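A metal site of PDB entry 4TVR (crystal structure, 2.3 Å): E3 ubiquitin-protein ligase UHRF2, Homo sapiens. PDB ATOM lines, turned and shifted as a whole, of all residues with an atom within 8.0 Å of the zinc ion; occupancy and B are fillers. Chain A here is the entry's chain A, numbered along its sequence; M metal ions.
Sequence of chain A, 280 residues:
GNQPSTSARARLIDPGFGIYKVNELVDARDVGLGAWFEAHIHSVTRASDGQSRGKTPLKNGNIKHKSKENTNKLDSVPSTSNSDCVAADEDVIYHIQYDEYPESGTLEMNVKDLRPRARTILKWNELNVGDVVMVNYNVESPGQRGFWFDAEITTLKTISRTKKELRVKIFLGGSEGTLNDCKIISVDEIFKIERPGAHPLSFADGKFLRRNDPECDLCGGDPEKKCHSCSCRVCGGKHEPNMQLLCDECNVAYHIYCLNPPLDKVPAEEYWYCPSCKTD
The zinc ion is bound by SG of Cys 247, SG of Cys 250 and SG of Cys 274.
SG of Cys 247 lies close to N of Glu 249, 3.6 Å away.
Of the 16 residues printed, 3 come within 4 Å of the zinc ion.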
ATOM      1  N   LEU A 246      -5.582 -16.281   3.490  1.00  0.00           N
ATOM      2  CA  LEU A 246      -5.561 -17.122   2.281  1.00  0.00           C
ATOM      3  C   LEU A 246      -5.728 -18.599   2.614  1.00  0.00           C
ATOM      4  O   LEU A 246      -5.695 -18.989   3.791  1.00  0.00           O
ATOM      5  CB  LEU A 246      -4.241 -16.928   1.520  1.00  0.00           C
ATOM      6  CG  LEU A 246      -4.079 -15.680   0.639  1.00  0.00           C
ATOM      7  CD1 LEU A 246      -4.109 -14.398   1.462  1.00  0.00           C
ATOM      8  CD2 LEU A 246      -2.781 -15.779  -0.139  1.00  0.00           C
ATOM      9  N   CYS A 247      -5.896 -19.412   1.573  1.00  0.00           N
ATOM     10  CA  CYS A 247      -5.974 -20.876   1.699  1.00  0.00           C
ATOM     11  C   CYS A 247      -4.767 -21.515   1.012  1.00  0.00           C
ATOM     12  O   CYS A 247      -4.156 -20.921   0.127  1.00  0.00           O
ATOM     13  CB  CYS A 247      -7.282 -21.376   1.068  1.00  0.00           C
ATOM     14  SG  CYS A 247      -7.530 -23.166   1.098  1.00  0.00           S
ATOM     15  N   ASP A 248      -4.418 -22.732   1.439  1.00  0.00           N
ATOM     16  CA  ASP A 248      -3.254 -23.445   0.900  1.00  0.00           C
ATOM     17  C   ASP A 248      -3.608 -24.458  -0.192  1.00  0.00           C
ATOM     18  O   ASP A 248      -2.849 -24.607  -1.152  1.00  0.00           O
ATOM     19  CB  ASP A 248      -2.507 -24.146   2.042  1.00  0.00           C
ATOM     20  N   GLU A 249      -4.741 -25.144  -0.047  1.00  0.00           N
ATOM     21  CA  GLU A 249      -5.145 -26.179  -1.003  1.00  0.00           C
ATOM     22  C   GLU A 249      -5.644 -25.580  -2.324  1.00  0.00           C
ATOM     23  O   GLU A 249      -5.093 -25.865  -3.381  1.00  0.00           O
ATOM     24  CB  GLU A 249      -6.233 -27.072  -0.389  1.00  0.00           C
ATOM     25  N   CYS A 250      -6.695 -24.760  -2.242  1.00  0.00           N
ATOM     26  CA  CYS A 250      -7.326 -24.168  -3.437  1.00  0.00           C
ATOM     27  C   CYS A 250      -6.825 -22.750  -3.739  1.00  0.00           C
ATOM     28  O   CYS A 250      -6.823 -22.325  -4.897  1.00  0.00           O
ATOM     29  CB  CYS A 250      -8.846 -24.157  -3.278  1.00  0.00           C
ATOM     30  SG  CYS A 250      -9.492 -22.889  -2.155  1.00  0.00           S
ATOM     31  N   ASN A 251      -6.424 -22.015  -2.693  1.00  0.00           N
ATOM     32  CA  ASN A 251      -5.841 -20.672  -2.805  1.00  0.00           C
ATOM     33  C   ASN A 251      -6.829 -19.581  -3.247  1.00  0.00           C
ATOM     34  O   ASN A 251      -6.722 -19.035  -4.342  1.00  0.00           O
ATOM     35  CB  ASN A 251      -4.586 -20.689  -3.708  1.00  0.00           C
ATOM     36  CG  ASN A 251      -3.655 -19.514  -3.457  1.00  0.00           C
ATOM     37  OD1 ASN A 251      -4.002 -18.558  -2.761  1.00  0.00           O
ATOM     38  ND2 ASN A 251      -2.456 -19.585  -4.020  1.00  0.00           N
ATOM     39  N   VAL A 252      -7.785 -19.289  -2.369  1.00  0.00           N
ATOM     40  CA  VAL A 252      -8.694 -18.145  -2.523  1.00  0.00           C
ATOM     41  C   VAL A 252      -8.881 -17.455  -1.155  1.00  0.00           C
ATOM     42  O   VAL A 252      -8.864 -18.112  -0.119  1.00  0.00           O
ATOM     43  CB  VAL A 252     -10.068 -18.557  -3.111  1.00  0.00           C
ATOM     44  CG1 VAL A 252      -9.885 -19.258  -4.457  1.00  0.00           C
ATOM     45  CG2 VAL A 252     -10.864 -19.429  -2.140  1.00  0.00           C
ATOM     46  N   ALA A 253      -9.071 -16.134  -1.173  1.00  0.00           N
ATOM     47  CA  ALA A 253      -9.056 -15.328   0.039  1.00  0.00           C
ATOM     48  C   ALA A 253     -10.440 -14.986   0.598  1.00  0.00           C
ATOM     49  O   ALA A 253     -11.453 -15.063  -0.108  1.00  0.00           O
ATOM     50  CB  ALA A 253      -8.255 -14.046  -0.196  1.00  0.00           C
ATOM     51  N   TYR A 254     -10.467 -14.606   1.873  1.00  0.00           N
ATOM     52  CA  TYR A 254     -11.678 -14.131   2.559  1.00  0.00           C
ATOM     53  C   TYR A 254     -11.288 -13.130   3.653  1.00  0.00           C
ATOM     54  O   TYR A 254     -10.279 -13.333   4.337  1.00  0.00           O
ATOM     55  CB  TYR A 254     -12.422 -15.304   3.210  1.00  0.00           C
ATOM     56  CG  TYR A 254     -13.171 -16.215   2.266  1.00  0.00           C
ATOM     57  CD1 TYR A 254     -12.560 -17.349   1.733  1.00  0.00           C
ATOM     58  CD2 TYR A 254     -14.494 -15.960   1.917  1.00  0.00           C
ATOM     59  CE1 TYR A 254     -13.241 -18.200   0.871  1.00  0.00           C
ATOM     60  CE2 TYR A 254     -15.182 -16.795   1.052  1.00  0.00           C
ATOM     61  CZ  TYR A 254     -14.550 -17.918   0.537  1.00  0.00           C
ATOM     62  OH  TYR A 254     -15.229 -18.760  -0.311  1.00  0.00           O
ATOM     63  N   TRP A 272      -3.868 -20.648   7.456  1.00  0.00           N
ATOM     64  CA  TRP A 272      -5.320 -20.796   7.555  1.00  0.00           C
ATOM     65  C   TRP A 272      -5.864 -21.575   6.353  1.00  0.00           C
ATOM     66  O   TRP A 272      -5.262 -21.572   5.283  1.00  0.00           O
ATOM     67  CB  TRP A 272      -5.991 -19.425   7.650  1.00  0.00           C
ATOM     68  CG  TRP A 272      -7.469 -19.483   7.939  1.00  0.00           C
ATOM     69  CD1 TRP A 272      -8.055 -19.811   9.127  1.00  0.00           C
ATOM     70  CD2 TRP A 272      -8.530 -19.200   7.027  1.00  0.00           C
ATOM     71  NE1 TRP A 272      -9.426 -19.763   9.009  1.00  0.00           N
ATOM     72  CE2 TRP A 272      -9.743 -19.388   7.724  1.00  0.00           C
ATOM     73  CE3 TRP A 272      -8.582 -18.813   5.680  1.00  0.00           C
ATOM     74  CZ2 TRP A 272     -10.987 -19.194   7.121  1.00  0.00           C
ATOM     75  CZ3 TRP A 272      -9.827 -18.631   5.085  1.00  0.00           C
ATOM     76  CH2 TRP A 272     -11.004 -18.820   5.811  1.00  0.00           C
ATOM     77  N   TYR A 273      -7.005 -22.236   6.560  1.00  0.00           N
ATOM     78  CA  TYR A 273      -7.686 -22.982   5.500  1.00  0.00           C
ATOM     79  C   TYR A 273      -9.164 -22.608   5.443  1.00  0.00           C
ATOM     80  O   TYR A 273      -9.768 -22.275   6.463  1.00  0.00           O
ATOM     81  CB  TYR A 273      -7.506 -24.485   5.727  1.00  0.00           C
ATOM     82  CG  TYR A 273      -6.078 -24.957   5.536  1.00  0.00           C
ATOM     83  CD1 TYR A 273      -5.641 -25.421   4.303  1.00  0.00           C
ATOM     84  CD2 TYR A 273      -5.164 -24.929   6.595  1.00  0.00           C
ATOM     85  CE1 TYR A 273      -4.337 -25.864   4.127  1.00  0.00           C
ATOM     86  CE2 TYR A 273      -3.861 -25.358   6.424  1.00  0.00           C
ATOM     87  CZ  TYR A 273      -3.458 -25.825   5.185  1.00  0.00           C
ATOM     88  OH  TYR A 273      -2.155 -26.254   5.014  1.00  0.00           O
ATOM     89  N   CYS A 274      -9.745 -22.686   4.240  1.00  0.00           N
ATOM     90  CA  CYS A 274     -11.106 -22.198   3.988  1.00  0.00           C
ATOM     91  C   CYS A 274     -12.190 -23.128   4.562  1.00  0.00           C
ATOM     92  O   CYS A 274     -11.988 -24.340   4.639  1.00  0.00           O
ATOM     93  CB  CYS A 274     -11.313 -21.978   2.491  1.00  0.00           C
ATOM     94  SG  CYS A 274     -11.423 -23.483   1.490  1.00  0.00           S
ATOM     95  N   PRO A 275     -13.352 -22.562   4.961  1.00  0.00           N
ATOM     96  CA  PRO A 275     -14.411 -23.333   5.607  1.00  0.00           C
ATOM     97  C   PRO A 275     -15.282 -24.154   4.651  1.00  0.00           C
ATOM     98  O   PRO A 275     -15.853 -25.163   5.050  1.00  0.00           O
ATOM     99  CB  PRO A 275     -15.261 -22.256   6.275  1.00  0.00           C
ATOM    100  CG  PRO A 275     -15.122 -21.077   5.381  1.00  0.00           C
ATOM    101  CD  PRO A 275     -13.712 -21.129   4.847  1.00  0.00           C
ATOM    102  N   SER A 276     -15.389 -23.713   3.390  1.00  0.00           N
ATOM    103  CA  SER A 276     -16.191 -24.408   2.387  1.00  0.00           C
ATOM    104  C   SER A 276     -15.609 -25.780   2.006  1.00  0.00           C
ATOM    105  O   SER A 276     -16.311 -26.622   1.443  1.00  0.00           O
ATOM    106  CB  SER A 276     -16.345 -23.546   1.132  1.00  0.00           C
ATOM    107  OG  SER A 276     -17.226 -24.136   0.199  1.00  0.00           O
ATOM    108  N   CYS A 277     -14.317 -25.988   2.294  1.00  0.00           N
ATOM    109  CA  CYS A 277     -13.682 -27.284   2.091  1.00  0.00           C
ATOM    110  C   CYS A 277     -14.134 -28.251   3.192  1.00  0.00           C
ATOM    111  O   CYS A 277     -14.642 -29.337   2.900  1.00  0.00           O
ATOM    112  CB  CYS A 277     -12.159 -27.140   2.108  1.00  0.00           C
ATOM    113  N   LYS A 278     -13.940 -27.845   4.446  1.00  0.00           N
ATOM    114  CA  LYS A 278     -14.369 -28.651   5.597  1.00  0.00           C
ATOM    115  C   LYS A 278     -15.799 -28.283   5.999  1.00  0.00           C
ATOM    116  O   LYS A 278     -16.142 -28.267   7.180  1.00  0.00           O
ATOM    117  CB  LYS A 278     -13.414 -28.430   6.779  1.00  0.00           C
HETATM  118 ZN    ZN M   1      -9.568 -23.665   0.060  1.00  0.00          ZN
